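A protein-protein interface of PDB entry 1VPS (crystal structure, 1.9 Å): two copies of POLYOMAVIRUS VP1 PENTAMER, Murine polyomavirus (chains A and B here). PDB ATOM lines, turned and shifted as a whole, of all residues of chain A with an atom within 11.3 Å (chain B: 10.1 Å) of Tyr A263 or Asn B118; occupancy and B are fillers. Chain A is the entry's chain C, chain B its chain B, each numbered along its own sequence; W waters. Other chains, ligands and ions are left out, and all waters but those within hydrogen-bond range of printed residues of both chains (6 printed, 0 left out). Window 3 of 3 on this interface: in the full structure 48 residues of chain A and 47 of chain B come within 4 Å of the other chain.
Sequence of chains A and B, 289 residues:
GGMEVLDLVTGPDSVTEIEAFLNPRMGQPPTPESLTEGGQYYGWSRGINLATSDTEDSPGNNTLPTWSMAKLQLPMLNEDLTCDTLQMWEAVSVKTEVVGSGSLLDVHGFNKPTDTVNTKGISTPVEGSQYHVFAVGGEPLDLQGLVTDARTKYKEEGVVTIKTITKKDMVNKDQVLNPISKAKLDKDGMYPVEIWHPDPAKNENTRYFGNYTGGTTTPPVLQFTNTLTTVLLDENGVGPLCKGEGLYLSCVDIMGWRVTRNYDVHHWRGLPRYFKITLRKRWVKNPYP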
ATOM      1  N   GLY A  47      -5.635  -0.656  15.589  1.00  0.00           N
ATOM      2  CA  GLY A  47      -5.433   0.496  16.462  1.00  0.00           C
ATOM      3  C   GLY A  47      -6.503   1.566  16.366  1.00  0.00           C
ATOM      4  O   GLY A  47      -6.801   2.042  15.275  1.00  0.00           O
ATOM      5  N   ILE A  48      -7.090   1.939  17.498  1.00  0.00           N
ATOM      6  CA  ILE A  48      -8.143   2.957  17.522  1.00  0.00           C
ATOM      7  C   ILE A  48      -7.582   4.326  17.108  1.00  0.00           C
ATOM      8  O   ILE A  48      -6.590   4.793  17.669  1.00  0.00           O
ATOM      9  CB  ILE A  48      -8.807   3.023  18.934  1.00  0.00           C
ATOM     10  CG1 ILE A  48      -9.578   1.721  19.206  1.00  0.00           C
ATOM     11  CG2 ILE A  48      -9.739   4.234  19.054  1.00  0.00           C
ATOM     12  CD1 ILE A  48     -10.002   1.551  20.649  1.00  0.00           C
ATOM     13  N   ASN A  49      -8.191   4.930  16.089  1.00  0.00           N
ATOM     14  CA  ASN A  49      -7.770   6.241  15.586  1.00  0.00           C
ATOM     15  C   ASN A  49      -8.724   7.332  16.104  1.00  0.00           C
ATOM     16  O   ASN A  49      -9.952   7.161  16.084  1.00  0.00           O
ATOM     17  CB  ASN A  49      -7.682   6.231  14.048  1.00  0.00           C
ATOM     18  CG  ASN A  49      -9.043   6.084  13.363  1.00  0.00           C
ATOM     19  OD1 ASN A  49      -9.756   5.089  13.551  1.00  0.00           O
ATOM     20  ND2 ASN A  49      -9.406   7.080  12.551  1.00  0.00           N
ATOM     21  N   LEU A  50      -8.157   8.435  16.593  1.00  0.00           N
ATOM     22  CA  LEU A  50      -8.939   9.526  17.171  1.00  0.00           C
ATOM     23  C   LEU A  50      -9.318  10.648  16.216  1.00  0.00           C
ATOM     24  O   LEU A  50      -8.649  10.882  15.214  1.00  0.00           O
ATOM     25  CB  LEU A  50      -8.195  10.136  18.365  1.00  0.00           C
ATOM     26  CG  LEU A  50      -7.646   9.205  19.452  1.00  0.00           C
ATOM     27  CD1 LEU A  50      -7.056  10.035  20.590  1.00  0.00           C
ATOM     28  CD2 LEU A  50      -8.749   8.288  19.970  1.00  0.00           C
ATOM     29  N   ALA A  51     -10.380  11.368  16.573  1.00  0.00           N
ATOM     30  CA  ALA A  51     -10.863  12.499  15.791  1.00  0.00           C
ATOM     31  C   ALA A  51      -9.769  13.568  15.741  1.00  0.00           C
ATOM     32  O   ALA A  51      -8.978  13.701  16.681  1.00  0.00           O
ATOM     33  CB  ALA A  51     -12.120  13.070  16.437  1.00  0.00           C
ATOM     34  N   PHE A 110       4.422  -7.892  24.712  1.00  0.00           N
ATOM     35  CA  PHE A 110       5.074  -6.611  24.454  1.00  0.00           C
ATOM     36  C   PHE A 110       4.141  -5.401  24.609  1.00  0.00           C
ATOM     37  O   PHE A 110       4.316  -4.395  23.916  1.00  0.00           O
ATOM     38  CB  PHE A 110       5.654  -6.642  23.029  1.00  0.00           C
ATOM     39  CG  PHE A 110       6.839  -5.729  22.815  1.00  0.00           C
ATOM     40  CD1 PHE A 110       8.001  -5.868  23.577  1.00  0.00           C
ATOM     41  CD2 PHE A 110       6.820  -4.773  21.801  1.00  0.00           C
ATOM     42  CE1 PHE A 110       9.134  -5.070  23.322  1.00  0.00           C
ATOM     43  CE2 PHE A 110       7.943  -3.971  21.537  1.00  0.00           C
ATOM     44  CZ  PHE A 110       9.102  -4.121  22.299  1.00  0.00           C
ATOM     45  N   ASN A 111       3.143  -5.492  25.489  1.00  0.00           N
ATOM     46  CA  ASN A 111       2.223  -4.371  25.700  1.00  0.00           C
ATOM     47  C   ASN A 111       2.952  -3.326  26.535  1.00  0.00           C
ATOM     48  O   ASN A 111       4.068  -3.559  27.002  1.00  0.00           O
ATOM     49  CB  ASN A 111       0.979  -4.801  26.499  1.00  0.00           C
ATOM     50  CG  ASN A 111       0.081  -5.767  25.744  1.00  0.00           C
ATOM     51  OD1 ASN A 111       0.189  -5.928  24.524  1.00  0.00           O
ATOM     52  ND2 ASN A 111      -0.818  -6.420  26.475  1.00  0.00           N
ATOM     53  N   LYS A 112       2.323  -2.170  26.710  1.00  0.00           N
ATOM     54  CA  LYS A 112       2.882  -1.113  27.545  1.00  0.00           C
ATOM     55  C   LYS A 112       3.183  -1.768  28.907  1.00  0.00           C
ATOM     56  O   LYS A 112       2.316  -2.425  29.494  1.00  0.00           O
ATOM     57  CB  LYS A 112       1.842  -0.003  27.702  1.00  0.00           C
ATOM     58  CG  LYS A 112       2.272   1.172  28.553  1.00  0.00           C
ATOM     59  CD  LYS A 112       1.131   2.183  28.633  1.00  0.00           C
ATOM     60  CE  LYS A 112       1.435   3.285  29.625  1.00  0.00           C
ATOM     61  NZ  LYS A 112       1.245   4.608  29.001  1.00  0.00           N
ATOM     62  N   PRO A 113       4.436  -1.663  29.381  1.00  0.00           N
ATOM     63  CA  PRO A 113       4.814  -2.264  30.666  1.00  0.00           C
ATOM     64  C   PRO A 113       4.303  -1.492  31.882  1.00  0.00           C
ATOM     65  O   PRO A 113       4.049  -0.290  31.802  1.00  0.00           O
ATOM     66  CB  PRO A 113       6.339  -2.271  30.593  1.00  0.00           C
ATOM     67  CG  PRO A 113       6.631  -1.021  29.825  1.00  0.00           C
ATOM     68  CD  PRO A 113       5.602  -1.039  28.724  1.00  0.00           C
ATOM     69  N   THR A 116       7.030   1.841  33.305  1.00  0.00           N
ATOM     70  CA  THR A 116       7.418   2.538  32.079  1.00  0.00           C
ATOM     71  C   THR A 116       8.753   3.273  32.167  1.00  0.00           C
ATOM     72  O   THR A 116       9.411   3.491  31.152  1.00  0.00           O
ATOM     73  CB  THR A 116       6.313   3.511  31.624  1.00  0.00           C
ATOM     74  OG1 THR A 116       6.069   4.472  32.657  1.00  0.00           O
ATOM     75  CG2 THR A 116       5.022   2.751  31.343  1.00  0.00           C
ATOM     76  N   TRP A 257      -9.401  -3.270  26.399  1.00  0.00           N
ATOM     77  CA  TRP A 257      -8.369  -2.969  25.404  1.00  0.00           C
ATOM     78  C   TRP A 257      -7.011  -3.376  25.927  1.00  0.00           C
ATOM     79  O   TRP A 257      -6.802  -3.448  27.137  1.00  0.00           O
ATOM     80  CB  TRP A 257      -8.210  -1.448  25.187  1.00  0.00           C
ATOM     81  CG  TRP A 257      -9.433  -0.653  24.876  1.00  0.00           C
ATOM     82  CD1 TRP A 257     -10.054  -0.543  23.661  1.00  0.00           C
ATOM     83  CD2 TRP A 257     -10.174   0.163  25.791  1.00  0.00           C
ATOM     84  NE1 TRP A 257     -11.145   0.293  23.766  1.00  0.00           N
ATOM     85  CE2 TRP A 257     -11.248   0.737  25.065  1.00  0.00           C
ATOM     86  CE3 TRP A 257     -10.050   0.472  27.152  1.00  0.00           C
ATOM     87  CZ2 TRP A 257     -12.186   1.592  25.653  1.00  0.00           C
ATOM     88  CZ3 TRP A 257     -10.984   1.328  27.739  1.00  0.00           C
ATOM     89  CH2 TRP A 257     -12.037   1.875  26.988  1.00  0.00           C
ATOM     90  N   ARG A 258      -6.084  -3.615  25.005  1.00  0.00           N
ATOM     91  CA  ARG A 258      -4.698  -3.842  25.378  1.00  0.00           C
ATOM     92  C   ARG A 258      -4.068  -2.549  24.817  1.00  0.00           C
ATOM     93  O   ARG A 258      -4.596  -1.954  23.864  1.00  0.00           O
ATOM     94  CB  ARG A 258      -4.101  -5.096  24.738  1.00  0.00           C
ATOM     95  CG  ARG A 258      -3.887  -5.028  23.254  1.00  0.00           C
ATOM     96  CD  ARG A 258      -2.953  -6.147  22.808  1.00  0.00           C
ATOM     97  NE  ARG A 258      -2.628  -5.987  21.399  1.00  0.00           N
ATOM     98  CZ  ARG A 258      -1.516  -5.412  20.943  1.00  0.00           C
ATOM     99  NH1 ARG A 258      -0.588  -4.950  21.782  1.00  0.00           N
ATOM    100  NH2 ARG A 258      -1.368  -5.245  19.637  1.00  0.00           N
ATOM    101  N   VAL A 259      -3.003  -2.075  25.443  1.00  0.00           N
ATOM    102  CA  VAL A 259      -2.338  -0.836  25.038  1.00  0.00           C
ATOM    103  C   VAL A 259      -0.894  -1.113  24.590  1.00  0.00           C
ATOM    104  O   VAL A 259      -0.142  -1.784  25.302  1.00  0.00           O
ATOM    105  CB  VAL A 259      -2.334   0.167  26.227  1.00  0.00           C
ATOM    106  CG1 VAL A 259      -1.770   1.519  25.802  1.00  0.00           C
ATOM    107  CG2 VAL A 259      -3.740   0.316  26.797  1.00  0.00           C
ATOM    108  N   THR A 260      -0.502  -0.605  23.422  1.00  0.00           N
ATOM    109  CA  THR A 260       0.856  -0.826  22.916  1.00  0.00           C
ATOM    110  C   THR A 260       1.890   0.124  23.543  1.00  0.00           C
ATOM    111  O   THR A 260       1.545   1.024  24.317  1.00  0.00           O
ATOM    112  CB  THR A 260       0.924  -0.686  21.375  1.00  0.00           C
ATOM    113  OG1 THR A 260       0.936   0.702  21.015  1.00  0.00           O
ATOM    114  CG2 THR A 260      -0.273  -1.380  20.711  1.00  0.00           C
ATOM    115  N   ARG A 261       3.162  -0.081  23.203  1.00  0.00           N
ATOM    116  CA  ARG A 261       4.247   0.761  23.706  1.00  0.00           C
ATOM    117  C   ARG A 261       4.436   1.998  22.834  1.00  0.00           C
ATOM    118  O   ARG A 261       5.293   2.830  23.108  1.00  0.00           O
ATOM    119  CB  ARG A 261       5.561  -0.030  23.767  1.00  0.00           C
ATOM    120  CG  ARG A 261       5.558  -1.148  24.797  1.00  0.00           C
ATOM    121  CD  ARG A 261       6.882  -1.891  24.796  1.00  0.00           C
ATOM    122  NE  ARG A 261       6.941  -2.928  25.825  1.00  0.00           N
ATOM    123  CZ  ARG A 261       8.064  -3.516  26.219  1.00  0.00           C
ATOM    124  NH1 ARG A 261       9.223  -3.168  25.679  1.00  0.00           N
ATOM    125  NH2 ARG A 261       8.026  -4.464  27.142  1.00  0.00           N
ATOM    126  N   ASN A 262       3.613   2.005  21.672  1.00  0.00           N
ATOM    127  CA  ASN A 262       3.734   3.102  20.719  1.00  0.00           C
ATOM    128  C   ASN A 262       2.573   4.076  20.862  1.00  0.00           C
ATOM    129  O   ASN A 262       1.477   3.809  20.365  1.00  0.00           O
ATOM    130  CB  ASN A 262       3.759   2.563  19.282  1.00  0.00           C
ATOM    131  CG  ASN A 262       4.657   1.346  19.120  1.00  0.00           C
ATOM    132  OD1 ASN A 262       5.869   1.413  19.374  1.00  0.00           O
ATOM    133  ND2 ASN A 262       4.071   0.222  18.691  1.00  0.00           N
ATOM    134  N   TYR A 263       2.667   5.336  21.524  1.00  0.00           N
ATOM    135  CA  TYR A 263       1.618   6.340  21.652  1.00  0.00           C
ATOM    136  C   TYR A 263       0.318   5.811  22.257  1.00  0.00           C
ATOM    137  O   TYR A 263      -0.773   6.251  21.884  1.00  0.00           O
ATOM    138  CB  TYR A 263       1.357   7.034  20.310  1.00  0.00           C
ATOM    139  CG  TYR A 263       2.538   7.849  19.818  1.00  0.00           C
ATOM    140  CD1 TYR A 263       3.212   8.728  20.673  1.00  0.00           C
ATOM    141  CD2 TYR A 263       3.000   7.726  18.505  1.00  0.00           C
ATOM    142  CE1 TYR A 263       4.322   9.465  20.233  1.00  0.00           C
ATOM    143  CE2 TYR A 263       4.109   8.459  18.053  1.00  0.00           C
ATOM    144  CZ  TYR A 263       4.765   9.325  18.923  1.00  0.00           C
ATOM    145  OH  TYR A 263       5.861  10.039  18.479  1.00  0.00           O
ATOM    146  N   ASP A 264       0.436   4.877  23.199  1.00  0.00           N
ATOM    147  CA  ASP A 264      -0.733   4.313  23.871  1.00  0.00           C
ATOM    148  C   ASP A 264      -1.852   3.836  22.930  1.00  0.00           C
ATOM    149  O   ASP A 264      -3.036   4.004  23.251  1.00  0.00           O
ATOM    150  CB  ASP A 264      -1.318   5.334  24.865  1.00  0.00           C
ATOM    151  CG  ASP A 264      -0.525   5.438  26.166  1.00  0.00           C
ATOM    152  OD1 ASP A 264       0.614   4.930  26.261  1.00  0.00           O
ATOM    153  OD2 ASP A 264      -1.055   6.042  27.116  1.00  0.00           O
ATOM    154  N   VAL A 265      -1.500   3.256  21.782  1.00  0.00           N
ATOM    155  CA  VAL A 265      -2.513   2.763  20.848  1.00  0.00           C
ATOM    156  C   VAL A 265      -3.315   1.623  21.515  1.00  0.00           C
ATOM    157  O   VAL A 265      -2.734   0.700  22.097  1.00  0.00           O
ATOM    158  CB  VAL A 265      -1.883   2.271  19.511  1.00  0.00           C
ATOM    159  CG1 VAL A 265      -2.940   1.584  18.641  1.00  0.00           C
ATOM    160  CG2 VAL A 265      -1.282   3.457  18.743  1.00  0.00           C
ATOM    161  N   HIS A 266      -4.642   1.732  21.470  1.00  0.00           N
ATOM    162  CA  HIS A 266      -5.523   0.739  22.071  1.00  0.00           C
ATOM    163  C   HIS A 266      -6.117  -0.188  21.022  1.00  0.00           C
ATOM    164  O   HIS A 266      -6.427   0.240  19.902  1.00  0.00           O
ATOM    165  CB  HIS A 266      -6.687   1.416  22.810  1.00  0.00           C
ATOM    166  CG  HIS A 266      -6.312   2.071  24.103  1.00  0.00           C
ATOM    167  ND1 HIS A 266      -5.274   2.976  24.212  1.00  0.00           N
ATOM    168  CD2 HIS A 266      -6.882   2.007  25.330  1.00  0.00           C
ATOM    169  CE1 HIS A 266      -5.228   3.446  25.453  1.00  0.00           C
ATOM    170  NE2 HIS A 266      -6.194   2.871  26.145  1.00  0.00           N
ATOM    171  N   HIS A 267      -6.269  -1.458  21.392  1.00  0.00           N
ATOM    172  CA  HIS A 267      -6.873  -2.471  20.525  1.00  0.00           C
ATOM    173  C   HIS A 267      -7.949  -3.161  21.352  1.00  0.00           C
ATOM    174  O   HIS A 267      -7.652  -3.668  22.437  1.00  0.00           O
ATOM    175  CB  HIS A 267      -5.852  -3.542  20.113  1.00  0.00           C
ATOM    176  CG  HIS A 267      -4.811  -3.059  19.151  1.00  0.00           C
ATOM    177  ND1 HIS A 267      -4.900  -3.271  17.792  1.00  0.00           N
ATOM    178  CD2 HIS A 267      -3.655  -2.381  19.348  1.00  0.00           C
ATOM    179  CE1 HIS A 267      -3.849  -2.744  17.194  1.00  0.00           C
ATOM    180  NE2 HIS A 267      -3.077  -2.194  18.115  1.00  0.00           N
ATOM    181  N   LYS B 112     -10.966  14.681  26.113  1.00  0.00           N
ATOM    182  CA  LYS B 112      -9.643  14.720  26.729  1.00  0.00           C
ATOM    183  C   LYS B 112      -9.042  13.327  26.478  1.00  0.00           C
ATOM    184  O   LYS B 112      -9.692  12.308  26.740  1.00  0.00           O
ATOM    185  CB  LYS B 112      -9.796  14.976  28.227  1.00  0.00           C
ATOM    186  CG  LYS B 112      -8.503  15.068  29.024  1.00  0.00           C
ATOM    187  CD  LYS B 112      -8.839  15.118  30.507  1.00  0.00           C
ATOM    188  CE  LYS B 112      -7.602  15.206  31.382  1.00  0.00           C
ATOM    189  NZ  LYS B 112      -6.920  16.500  31.178  1.00  0.00           N
ATOM    190  N   PRO B 113      -7.826  13.265  25.909  1.00  0.00           N
ATOM    191  CA  PRO B 113      -7.197  11.969  25.629  1.00  0.00           C
ATOM    192  C   PRO B 113      -6.564  11.313  26.859  1.00  0.00           C
ATOM    193  O   PRO B 113      -6.205  12.002  27.815  1.00  0.00           O
ATOM    194  CB  PRO B 113      -6.150  12.335  24.576  1.00  0.00           C
ATOM    195  CG  PRO B 113      -5.687  13.691  25.048  1.00  0.00           C
ATOM    196  CD  PRO B 113      -6.976  14.385  25.447  1.00  0.00           C
ATOM    197  N   THR B 114      -6.415   9.991  26.824  1.00  0.00           N
ATOM    198  CA  THR B 114      -5.817   9.261  27.939  1.00  0.00           C
ATOM    199  C   THR B 114      -4.290   9.454  28.049  1.00  0.00           C
ATOM    200  O   THR B 114      -3.705   9.242  29.115  1.00  0.00           O
ATOM    201  CB  THR B 114      -6.196   7.751  27.916  1.00  0.00           C
ATOM    202  OG1 THR B 114      -5.844   7.173  26.651  1.00  0.00           O
ATOM    203  CG2 THR B 114      -7.688   7.577  28.162  1.00  0.00           C
ATOM    204  N   ASP B 115      -3.646   9.812  26.942  1.00  0.00           N
ATOM    205  CA  ASP B 115      -2.207  10.083  26.934  1.00  0.00           C
ATOM    206  C   ASP B 115      -2.094  11.597  26.725  1.00  0.00           C
ATOM    207  O   ASP B 115      -2.125  12.086  25.592  1.00  0.00           O
ATOM    208  CB  ASP B 115      -1.514   9.322  25.789  1.00  0.00           C
ATOM    209  CG  ASP B 115      -0.024   9.683  25.627  1.00  0.00           C
ATOM    210  OD1 ASP B 115       0.527  10.497  26.408  1.00  0.00           O
ATOM    211  OD2 ASP B 115       0.602   9.143  24.691  1.00  0.00           O
ATOM    212  N   THR B 116      -1.957  12.332  27.819  1.00  0.00           N
ATOM    213  CA  THR B 116      -1.867  13.785  27.755  1.00  0.00           C
ATOM    214  C   THR B 116      -0.490  14.320  27.382  1.00  0.00           C
ATOM    215  O   THR B 116      -0.362  15.492  27.029  1.00  0.00           O
ATOM    216  CB  THR B 116      -2.359  14.436  29.062  1.00  0.00           C
ATOM    217  OG1 THR B 116      -1.681  13.852  30.183  1.00  0.00           O
ATOM    218  CG2 THR B 116      -3.866  14.235  29.216  1.00  0.00           C
ATOM    219  N   VAL B 117       0.536  13.475  27.461  1.00  0.00           N
ATOM    220  CA  VAL B 117       1.885  13.899  27.087  1.00  0.00           C
ATOM    221  C   VAL B 117       1.990  14.070  25.577  1.00  0.00           C
ATOM    222  O   VAL B 117       2.557  15.049  25.090  1.00  0.00           O
ATOM    223  CB  VAL B 117       2.951  12.869  27.534  1.00  0.00           C
ATOM    224  CG1 VAL B 117       4.329  13.234  26.982  1.00  0.00           C
ATOM    225  CG2 VAL B 117       2.975  12.773  29.040  1.00  0.00           C
ATOM    226  N   ASN B 118       1.420  13.116  24.848  1.00  0.00           N
ATOM    227  CA  ASN B 118       1.459  13.118  23.393  1.00  0.00           C
ATOM    228  C   ASN B 118       0.124  13.438  22.726  1.00  0.00           C
ATOM    229  O   ASN B 118       0.082  13.589  21.507  1.00  0.00           O
ATOM    230  CB  ASN B 118       1.931  11.745  22.895  1.00  0.00           C
ATOM    231  CG  ASN B 118       3.339  11.391  23.374  1.00  0.00           C
ATOM    232  OD1 ASN B 118       4.311  12.105  23.096  1.00  0.00           O
ATOM    233  ND2 ASN B 118       3.437  10.323  24.161  1.00  0.00           N
ATOM    234  N   THR B 119      -0.943  13.564  23.520  1.00  0.00           N
ATOM    235  CA  THR B 119      -2.303  13.796  23.018  1.00  0.00           C
ATOM    236  C   THR B 119      -2.661  12.586  22.130  1.00  0.00           C
ATOM    237  O   THR B 119      -2.952  12.710  20.932  1.00  0.00           O
ATOM    238  CB  THR B 119      -2.447  15.148  22.261  1.00  0.00           C
ATOM    239  OG1 THR B 119      -2.043  16.222  23.124  1.00  0.00           O
ATOM    240  CG2 THR B 119      -3.905  15.392  21.862  1.00  0.00           C
ATOM    241  N   LYS B 120      -2.609  11.409  22.754  1.00  0.00           N
ATOM    242  CA  LYS B 120      -2.873  10.131  22.096  1.00  0.00           C
ATOM    243  C   LYS B 120      -3.702   9.223  23.014  1.00  0.00           C
ATOM    244  O   LYS B 120      -4.288   9.691  23.995  1.00  0.00           O
ATOM    245  CB  LYS B 120      -1.542   9.430  21.783  1.00  0.00           C
ATOM    246  CG  LYS B 120      -0.607  10.183  20.860  1.00  0.00           C
ATOM    247  CD  LYS B 120      -1.079  10.161  19.432  1.00  0.00           C
ATOM    248  CE  LYS B 120      -0.027  10.780  18.539  1.00  0.00           C
ATOM    249  NZ  LYS B 120      -0.388  10.732  17.106  1.00  0.00           N
ATOM    250  N   GLY B 121      -3.677   7.917  22.733  1.00  0.00           N
ATOM    251  CA  GLY B 121      -4.423   6.951  23.524  1.00  0.00           C
ATOM    252  C   GLY B 121      -5.818   6.845  22.957  1.00  0.00           C
ATOM    253  O   GLY B 121      -5.978   6.570  21.769  1.00  0.00           O
ATOM    254  N   ILE B 122      -6.826   7.037  23.796  1.00  0.00           N
ATOM    255  CA  ILE B 122      -8.212   7.009  23.342  1.00  0.00           C
ATOM    256  C   ILE B 122      -8.914   8.248  23.883  1.00  0.00           C
ATOM    257  O   ILE B 122      -8.386   8.953  24.752  1.00  0.00           O
ATOM    258  CB  ILE B 122      -8.999   5.749  23.835  1.00  0.00           C
ATOM    259  CG1 ILE B 122      -8.906   5.611  25.357  1.00  0.00           C
ATOM    260  CG2 ILE B 122      -8.517   4.493  23.124  1.00  0.00           C
ATOM    261  CD1 ILE B 122      -9.832   4.558  25.937  1.00  0.00           C
ATOM    262  N   SER B 123     -10.086   8.534  23.329  1.00  0.00           N
ATOM    263  CA  SER B 123     -10.906   9.653  23.775  1.00  0.00           C
ATOM    264  C   SER B 123     -11.546   9.124  25.068  1.00  0.00           C
ATOM    265  O   SER B 123     -12.243   8.108  25.043  1.00  0.00           O
ATOM    266  CB  SER B 123     -11.974   9.933  22.714  1.00  0.00           C
ATOM    267  OG  SER B 123     -12.793  11.023  23.069  1.00  0.00           O
ATOM    268  N   ARG B 261     -11.188  18.770  25.750  1.00  0.00           N
ATOM    269  CA  ARG B 261      -9.770  19.093  25.760  1.00  0.00           C
ATOM    270  C   ARG B 261      -9.527  20.546  26.171  1.00  0.00           C
ATOM    271  O   ARG B 261      -8.379  20.997  26.239  1.00  0.00           O
ATOM    272  CB  ARG B 261      -9.169  18.842  24.378  1.00  0.00           C
ATOM    273  CG  ARG B 261      -9.167  17.381  23.960  1.00  0.00           C
ATOM    274  CD  ARG B 261      -8.540  17.224  22.599  1.00  0.00           C
ATOM    275  NE  ARG B 261      -8.438  15.829  22.194  1.00  0.00           N
ATOM    276  CZ  ARG B 261      -7.606  15.389  21.255  1.00  0.00           C
ATOM    277  NH1 ARG B 261      -6.799  16.232  20.619  1.00  0.00           N
ATOM    278  NH2 ARG B 261      -7.587  14.105  20.940  1.00  0.00           N
HETATM  279  O   HOH W   1      -0.817   7.838  29.467  1.00  0.00           O
HETATM  280  O   HOH W   2      -2.791   6.491  20.092  1.00  0.00           O
HETATM  281  O   HOH W   3      -5.560   4.310  20.294  1.00  0.00           O
HETATM  282  O   HOH W   4      -3.796   5.552  27.365  1.00  0.00           O
HETATM  283  O   HOH W   5       2.628   7.470  24.188  1.00  0.00           O
HETATM  284  O   HOH W   6      -6.586  13.603  18.090  1.00  0.00           O
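N of Gly B121 sits at hydrogen-bond distance from O of Tyr A263 (3.5 Å).
The side-chain carboxylate of Asp A264 is in salt-bridge range of the side-chain amino group of Lys A112, at 2.8 Å. The backbone carbonyl oxygen of Asp A264 is in hydrogen-bond range of a ring nitrogen (ND1) of His A266. The side-chain carboxylate of Asp B115 sits at hydrogen-bond distance from the backbone NH of Val B117, at 3.2 Å. O of Asp B115 is in hydrogen-bond range of N of Lys B120 (3.0 Å). The side-chain amide nitrogen (ND2) of Asn B118 lies within hydrogen-bond range of the side-chain carboxylate (OD2) of Asp B115, at 3.1 Å. The backbone NH of Ile B122 sits at hydrogen-bond distance from the side-chain hydroxyl of Thr B114 (3.0 Å).
CD2 of Leu A50 touches O of Gly B121, at 3.7 Å. Leu A50 touches Ile B122 (CD2 to CA, 3.6 Å). Leu A50 touches Ser B123. Trp A257 touches Ile B122. CG of Asn B118 touches CD1 of Tyr A263, at 3.8 Å. Lys B120 touches Tyr A263 (CB to O, 3.3 Å). OD2 of Asp A264 touches CB of Asp B115, 3.6 Å away. Gly B121 touches Asp A264 (CA to O, 3.3 Å). OG1 of Thr B114 touches CE1 of His A266, at 3.96 Å. Ile B122 touches His A266.
Printed residues of chain B within 4 Å of Trp A257: Ile B122. No residue of chain B comes within 4 Å of Asn A262. Tyr A263 touches just these residues of chain B: Asn B118 (3.8 Å), Lys B120 (3.3 Å) and Gly B121 (3.5 Å). Of chain B, only Asp B115 (3.6 Å) and Gly B121 (3.3 Å) come within 4 Å of Asp A264. Printed residues of chain B within 4 Å of His A266: Thr B114 and Ile B122. Of the printed residues of chain A, Thr B114 touches His A266. No residue of chain A comes within 4 Å of Thr B116. No residue of chain A comes within 4 Å of Val B117. Of chain A, only Tyr A263 (3.8 Å) comes within 4 Å of Asn B118. No residue of chain A comes within 4 Å of Thr B119. Of chain A, only Leu A50 (3.7 Å), Tyr A263 (3.5 Å) and Asp A264 (3.3 Å) come within 4 Å of Gly B121. The nearest residue of chain A that does not touch Asn B118 is Asp A264 (6.3 Å).
Hydrophobic or aromatic side chains of chain A that line the printed part of chain B: Leu A50, Trp A257, Tyr A263 and His A266.
Positions printed for both chains: 112, 113, 116 and 261.
Water W5 lies within hydrogen-bond range of OD2 of Asp B115, ND2 of Asn B118 and N of Tyr A263. Water W4 bridges OG1 of Thr B114 (2.7 Å) and OD2 of Asp A264 (2.8 Å). Water W2 bridges the backbone carbonyl oxygen (O) of Tyr A263 and the backbone NH (N) of Gly B121. Water W3 lies within hydrogen-bond range of O of Gly B121 (2.7 Å), O of Ile A48 (2.9 Å) and N of His A266 (3.0 Å). Water W6 lies within hydrogen-bond range of O of Ala A51 (2.8 Å) and NH2 of Arg B261 (3.1 Å). Water W1 bridges OD2 of Asp A264 (3.0 Å) and O of Thr B114 (3.2 Å).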
